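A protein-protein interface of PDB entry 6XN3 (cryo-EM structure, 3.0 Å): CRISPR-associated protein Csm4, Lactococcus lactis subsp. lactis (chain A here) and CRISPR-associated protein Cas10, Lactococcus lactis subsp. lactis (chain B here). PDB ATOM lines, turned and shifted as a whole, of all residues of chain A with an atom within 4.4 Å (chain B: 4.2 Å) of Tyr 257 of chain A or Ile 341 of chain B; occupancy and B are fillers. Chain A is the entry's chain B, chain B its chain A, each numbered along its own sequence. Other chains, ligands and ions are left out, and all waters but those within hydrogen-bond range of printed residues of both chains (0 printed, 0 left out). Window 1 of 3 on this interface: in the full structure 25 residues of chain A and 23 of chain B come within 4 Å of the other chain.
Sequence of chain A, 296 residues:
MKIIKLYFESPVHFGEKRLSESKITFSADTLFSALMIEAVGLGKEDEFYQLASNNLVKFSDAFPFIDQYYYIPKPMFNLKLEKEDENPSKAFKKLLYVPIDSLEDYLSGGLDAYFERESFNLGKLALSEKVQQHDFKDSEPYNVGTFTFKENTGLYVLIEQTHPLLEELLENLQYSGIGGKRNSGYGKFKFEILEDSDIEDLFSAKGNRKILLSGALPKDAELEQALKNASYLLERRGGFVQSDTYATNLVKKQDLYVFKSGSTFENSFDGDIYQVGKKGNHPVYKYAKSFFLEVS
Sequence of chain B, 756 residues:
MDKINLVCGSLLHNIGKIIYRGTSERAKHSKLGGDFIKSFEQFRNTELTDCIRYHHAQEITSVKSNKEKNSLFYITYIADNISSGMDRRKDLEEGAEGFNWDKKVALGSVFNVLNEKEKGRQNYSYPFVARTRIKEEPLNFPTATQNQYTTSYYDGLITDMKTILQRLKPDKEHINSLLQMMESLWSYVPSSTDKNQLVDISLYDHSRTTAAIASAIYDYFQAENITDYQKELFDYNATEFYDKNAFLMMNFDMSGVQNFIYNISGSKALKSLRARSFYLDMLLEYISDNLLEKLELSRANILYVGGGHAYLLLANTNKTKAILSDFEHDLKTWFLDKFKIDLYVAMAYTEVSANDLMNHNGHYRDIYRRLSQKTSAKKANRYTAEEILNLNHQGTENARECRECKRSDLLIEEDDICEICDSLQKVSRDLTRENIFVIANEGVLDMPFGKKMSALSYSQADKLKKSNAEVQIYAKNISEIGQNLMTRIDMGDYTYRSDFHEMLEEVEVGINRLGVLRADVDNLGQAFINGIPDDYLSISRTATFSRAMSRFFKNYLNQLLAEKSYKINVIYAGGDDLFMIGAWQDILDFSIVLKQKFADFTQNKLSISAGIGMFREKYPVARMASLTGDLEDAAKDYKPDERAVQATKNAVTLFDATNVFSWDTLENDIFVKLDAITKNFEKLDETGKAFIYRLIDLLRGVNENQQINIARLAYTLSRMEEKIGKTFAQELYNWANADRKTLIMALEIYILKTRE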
ATOM      1  N   LEU A 217     -18.677   9.802  15.209  1.00  0.00           N
ATOM      2  CA  LEU A 217     -19.166   8.864  14.213  1.00  0.00           C
ATOM      3  C   LEU A 217     -19.587   7.590  14.923  1.00  0.00           C
ATOM      4  O   LEU A 217     -18.785   7.004  15.656  1.00  0.00           O
ATOM      5  CB  LEU A 217     -18.091   8.553  13.179  1.00  0.00           C
ATOM      6  CG  LEU A 217     -18.497   7.517  12.135  1.00  0.00           C
ATOM      7  CD1 LEU A 217     -19.396   8.156  11.103  1.00  0.00           C
ATOM      8  CD2 LEU A 217     -17.287   6.890  11.476  1.00  0.00           C
ATOM      9  N   LEU A 234     -21.001  15.852   7.159  1.00  0.00           N
ATOM     10  CA  LEU A 234     -19.753  15.138   7.322  1.00  0.00           C
ATOM     11  C   LEU A 234     -18.596  16.116   7.249  1.00  0.00           C
ATOM     12  O   LEU A 234     -18.690  17.191   6.654  1.00  0.00           O
ATOM     13  CB  LEU A 234     -19.582  14.061   6.253  1.00  0.00           C
ATOM     14  CG  LEU A 234     -20.206  12.668   6.363  1.00  0.00           C
ATOM     15  CD1 LEU A 234     -19.618  11.938   7.542  1.00  0.00           C
ATOM     16  CD2 LEU A 234     -21.701  12.685   6.461  1.00  0.00           C
ATOM     17  N   GLU A 235     -17.497  15.739   7.881  1.00  0.00           N
ATOM     18  CA  GLU A 235     -16.233  16.428   7.709  1.00  0.00           C
ATOM     19  C   GLU A 235     -15.186  15.362   7.475  1.00  0.00           C
ATOM     20  O   GLU A 235     -15.171  14.358   8.191  1.00  0.00           O
ATOM     21  CB  GLU A 235     -15.877  17.270   8.932  1.00  0.00           C
ATOM     22  CG  GLU A 235     -16.348  18.707   8.881  1.00  0.00           C
ATOM     23  CD  GLU A 235     -16.255  19.389  10.235  1.00  0.00           C
ATOM     24  OE1 GLU A 235     -16.742  20.530  10.371  1.00  0.00           O
ATOM     25  OE2 GLU A 235     -15.704  18.775  11.171  1.00  0.00           O
ATOM     26  N   ARG A 236     -14.339  15.549   6.468  1.00  0.00           N
ATOM     27  CA  ARG A 236     -13.187  14.673   6.354  1.00  0.00           C
ATOM     28  C   ARG A 236     -12.249  14.998   7.496  1.00  0.00           C
ATOM     29  O   ARG A 236     -12.206  16.136   7.974  1.00  0.00           O
ATOM     30  CB  ARG A 236     -12.466  14.826   5.023  1.00  0.00           C
ATOM     31  CG  ARG A 236     -11.813  16.146   4.780  1.00  0.00           C
ATOM     32  CD  ARG A 236     -11.181  16.131   3.419  1.00  0.00           C
ATOM     33  NE  ARG A 236     -10.091  15.159   3.406  1.00  0.00           N
ATOM     34  CZ  ARG A 236      -8.854  15.404   3.816  1.00  0.00           C
ATOM     35  NH1 ARG A 236      -8.526  16.595   4.292  1.00  0.00           N
ATOM     36  NH2 ARG A 236      -7.943  14.445   3.761  1.00  0.00           N
ATOM     37  N   ASP A 255      -8.490   8.601   6.158  1.00  0.00           N
ATOM     38  CA  ASP A 255      -9.327   9.785   6.349  1.00  0.00           C
ATOM     39  C   ASP A 255     -10.699   9.366   6.861  1.00  0.00           C
ATOM     40  O   ASP A 255     -11.595   9.009   6.098  1.00  0.00           O
ATOM     41  CB  ASP A 255      -9.420  10.606   5.065  1.00  0.00           C
ATOM     42  CG  ASP A 255      -9.718   9.769   3.838  1.00  0.00           C
ATOM     43  OD1 ASP A 255      -9.686   8.526   3.945  1.00  0.00           O
ATOM     44  OD2 ASP A 255      -9.973  10.358   2.766  1.00  0.00           O
ATOM     45  N   LEU A 256     -10.849   9.386   8.174  1.00  0.00           N
ATOM     46  CA  LEU A 256     -12.122   9.087   8.801  1.00  0.00           C
ATOM     47  C   LEU A 256     -13.075  10.246   8.566  1.00  0.00           C
ATOM     48  O   LEU A 256     -12.663  11.404   8.555  1.00  0.00           O
ATOM     49  CB  LEU A 256     -11.913   8.856  10.295  1.00  0.00           C
ATOM     50  CG  LEU A 256     -13.096   8.464  11.161  1.00  0.00           C
ATOM     51  CD1 LEU A 256     -13.623   7.137  10.691  1.00  0.00           C
ATOM     52  CD2 LEU A 256     -12.658   8.382  12.596  1.00  0.00           C
ATOM     53  N   TYR A 257     -14.347   9.939   8.358  1.00  0.00           N
ATOM     54  CA  TYR A 257     -15.355  10.965   8.138  1.00  0.00           C
ATOM     55  C   TYR A 257     -16.333  10.957   9.298  1.00  0.00           C
ATOM     56  O   TYR A 257     -17.073   9.988   9.483  1.00  0.00           O
ATOM     57  CB  TYR A 257     -16.098  10.749   6.827  1.00  0.00           C
ATOM     58  CG  TYR A 257     -15.311  11.106   5.600  1.00  0.00           C
ATOM     59  CD1 TYR A 257     -14.336  10.259   5.111  1.00  0.00           C
ATOM     60  CD2 TYR A 257     -15.588  12.260   4.892  1.00  0.00           C
ATOM     61  CE1 TYR A 257     -13.633  10.567   3.974  1.00  0.00           C
ATOM     62  CE2 TYR A 257     -14.890  12.576   3.757  1.00  0.00           C
ATOM     63  CZ  TYR A 257     -13.913  11.731   3.305  1.00  0.00           C
ATOM     64  OH  TYR A 257     -13.212  12.049   2.169  1.00  0.00           O
ATOM     65  N   VAL A 258     -16.358  12.049  10.053  1.00  0.00           N
ATOM     66  CA  VAL A 258     -17.130  12.131  11.278  1.00  0.00           C
ATOM     67  C   VAL A 258     -18.190  13.202  11.110  1.00  0.00           C
ATOM     68  O   VAL A 258     -18.124  14.035  10.207  1.00  0.00           O
ATOM     69  CB  VAL A 258     -16.236  12.443  12.488  1.00  0.00           C
ATOM     70  CG1 VAL A 258     -15.222  11.335  12.688  1.00  0.00           C
ATOM     71  CG2 VAL A 258     -15.535  13.760  12.284  1.00  0.00           C
ATOM     72  N   PHE B 339     -15.840  13.667  -6.034  1.00  0.00           N
ATOM     73  CA  PHE B 339     -15.616  14.676  -5.008  1.00  0.00           C
ATOM     74  C   PHE B 339     -16.258  14.170  -3.724  1.00  0.00           C
ATOM     75  O   PHE B 339     -17.475  14.284  -3.560  1.00  0.00           O
ATOM     76  CB  PHE B 339     -16.210  16.018  -5.421  1.00  0.00           C
ATOM     77  CG  PHE B 339     -15.993  16.363  -6.860  1.00  0.00           C
ATOM     78  CD1 PHE B 339     -14.789  16.887  -7.286  1.00  0.00           C
ATOM     79  CD2 PHE B 339     -17.001  16.174  -7.790  1.00  0.00           C
ATOM     80  CE1 PHE B 339     -14.596  17.211  -8.613  1.00  0.00           C
ATOM     81  CE2 PHE B 339     -16.810  16.492  -9.117  1.00  0.00           C
ATOM     82  CZ  PHE B 339     -15.604  17.009  -9.528  1.00  0.00           C
ATOM     83  N   LYS B 340     -15.428  13.667  -2.804  1.00  0.00           N
ATOM     84  CA  LYS B 340     -15.826  12.813  -1.687  1.00  0.00           C
ATOM     85  C   LYS B 340     -16.936  13.381  -0.809  1.00  0.00           C
ATOM     86  O   LYS B 340     -17.939  12.706  -0.573  1.00  0.00           O
ATOM     87  CB  LYS B 340     -14.606  12.515  -0.822  1.00  0.00           C
ATOM     88  CG  LYS B 340     -13.493  11.780  -1.541  1.00  0.00           C
ATOM     89  CD  LYS B 340     -13.822  10.319  -1.745  1.00  0.00           C
ATOM     90  CE  LYS B 340     -12.590   9.556  -2.189  1.00  0.00           C
ATOM     91  NZ  LYS B 340     -12.842   8.095  -2.295  1.00  0.00           N
ATOM     92  N   ILE B 341     -16.782  14.610  -0.321  1.00  0.00           N
ATOM     93  CA  ILE B 341     -17.902  15.331   0.278  1.00  0.00           C
ATOM     94  C   ILE B 341     -17.943  16.743  -0.278  1.00  0.00           C
ATOM     95  O   ILE B 341     -18.765  17.559   0.150  1.00  0.00           O
ATOM     96  CB  ILE B 341     -17.834  15.388   1.817  1.00  0.00           C
ATOM     97  CG1 ILE B 341     -16.624  16.200   2.268  1.00  0.00           C
ATOM     98  CG2 ILE B 341     -17.896  14.015   2.453  1.00  0.00           C
ATOM     99  CD1 ILE B 341     -16.826  16.885   3.590  1.00  0.00           C
ATOM    100  N   ASP B 342     -17.047  17.043  -1.222  1.00  0.00           N
ATOM    101  CA  ASP B 342     -16.832  18.427  -1.639  1.00  0.00           C
ATOM    102  C   ASP B 342     -18.018  18.998  -2.400  1.00  0.00           C
ATOM    103  O   ASP B 342     -18.428  20.133  -2.135  1.00  0.00           O
ATOM    104  CB  ASP B 342     -15.575  18.529  -2.496  1.00  0.00           C
ATOM    105  CG  ASP B 342     -14.344  18.047  -1.771  1.00  0.00           C
ATOM    106  OD1 ASP B 342     -14.482  17.591  -0.618  1.00  0.00           O
ATOM    107  OD2 ASP B 342     -13.240  18.127  -2.351  1.00  0.00           O
ATOM    108  N   LEU B 343     -18.587  18.243  -3.329  1.00  0.00           N
ATOM    109  CA  LEU B 343     -19.677  18.739  -4.150  1.00  0.00           C
ATOM    110  C   LEU B 343     -20.931  17.920  -3.901  1.00  0.00           C
ATOM    111  O   LEU B 343     -20.872  16.698  -3.749  1.00  0.00           O
ATOM    112  CB  LEU B 343     -19.340  18.706  -5.642  1.00  0.00           C
ATOM    113  CG  LEU B 343     -18.544  19.876  -6.224  1.00  0.00           C
ATOM    114  CD1 LEU B 343     -19.356  21.131  -6.029  1.00  0.00           C
ATOM    115  CD2 LEU B 343     -17.136  20.041  -5.694  1.00  0.00           C
ATOM    116  N   TYR B 383     -26.315  12.215   3.059  1.00  0.00           N
ATOM    117  CA  TYR B 383     -26.000  10.876   2.604  1.00  0.00           C
ATOM    118  C   TYR B 383     -26.723   9.858   3.468  1.00  0.00           C
ATOM    119  O   TYR B 383     -27.026  10.107   4.635  1.00  0.00           O
ATOM    120  CB  TYR B 383     -24.491  10.639   2.644  1.00  0.00           C
ATOM    121  CG  TYR B 383     -23.700  11.837   2.179  1.00  0.00           C
ATOM    122  CD1 TYR B 383     -23.748  12.255   0.861  1.00  0.00           C
ATOM    123  CD2 TYR B 383     -22.912  12.552   3.063  1.00  0.00           C
ATOM    124  CE1 TYR B 383     -23.032  13.350   0.439  1.00  0.00           C
ATOM    125  CE2 TYR B 383     -22.194  13.647   2.650  1.00  0.00           C
ATOM    126  CZ  TYR B 383     -22.257  14.041   1.337  1.00  0.00           C
ATOM    127  OH  TYR B 383     -21.543  15.134   0.917  1.00  0.00           O
ATOM    128  N   LEU B 391     -18.051   5.224   2.317  1.00  0.00           N
ATOM    129  CA  LEU B 391     -17.166   6.376   2.268  1.00  0.00           C
ATOM    130  C   LEU B 391     -16.104   6.324   3.357  1.00  0.00           C
ATOM    131  O   LEU B 391     -15.017   6.886   3.194  1.00  0.00           O
ATOM    132  CB  LEU B 391     -18.038   7.624   2.348  1.00  0.00           C
ATOM    133  CG  LEU B 391     -17.565   9.054   2.236  1.00  0.00           C
ATOM    134  CD1 LEU B 391     -18.627   9.887   1.633  1.00  0.00           C
ATOM    135  CD2 LEU B 391     -17.522   9.464   3.630  1.00  0.00           C
ATOM    136  N   ASN B 392     -16.398   5.669   4.474  1.00  0.00           N
ATOM    137  CA  ASN B 392     -15.358   5.453   5.476  1.00  0.00           C
ATOM    138  C   ASN B 392     -14.538   4.206   5.179  1.00  0.00           C
ATOM    139  O   ASN B 392     -13.355   4.150   5.522  1.00  0.00           O
ATOM    140  CB  ASN B 392     -15.971   5.362   6.868  1.00  0.00           C
ATOM    141  CG  ASN B 392     -16.087   6.704   7.534  1.00  0.00           C
ATOM    142  OD1 ASN B 392     -15.118   7.453   7.612  1.00  0.00           O
ATOM    143  ND2 ASN B 392     -17.277   7.029   8.003  1.00  0.00           N
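Of the printed residues of chain B, Tyr 257 of chain A touches Lys 340, Ile 341, Leu 391 and Asn 392. Ile 341 of chain B touches two residues of chain A. Of the printed residues of chain A, Asn 392 of chain B touches Leu 217 (3.5 Å), Leu 256 (3.4 Å) and Tyr 257 (2.7 Å). Printed residues of chain A within 4 Å of Leu 391 of chain B: Tyr 257 (3.4 Å). Printed residues of chain A within 4 Å of Tyr 383 of chain B: Leu 234. Of the printed residues of chain B, Leu 217 of chain A touches Asn 392 (3.5 Å).
The side-chain amide oxygen of Asn 392 of chain B lies within hydrogen-bond range of the backbone NH of Tyr 257 of chain A, at 2.7 Å.
Among the printed residues, merely in contact across the chains: Leu 217 of chain A with Asn 392 of chain B, Leu 234 of chain A with Ile 341 of chain B, Leu 234 of chain A with Tyr 383 of chain B, Leu 256 of chain A with Asn 392 of chain B, Tyr 257 of chain A with Lys 340 of chain B, Tyr 257 of chain A with Ile 341 of chain B and Tyr 257 of chain A with Leu 391 of chain B.
Printed residues of chain B that touch a printed residue of chain A: Lys 340, Ile 341, Tyr 383, Leu 391 and Asn 392. Hydrophobic or aromatic side chains of chain B within 4 Å of the printed part of chain A: Ile 341, Tyr 383 and Leu 391. Of the 8 printed residues of chain A, 4 touch a printed residue of chain B. Among the printed residues, 8 pairs touch across the chains.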
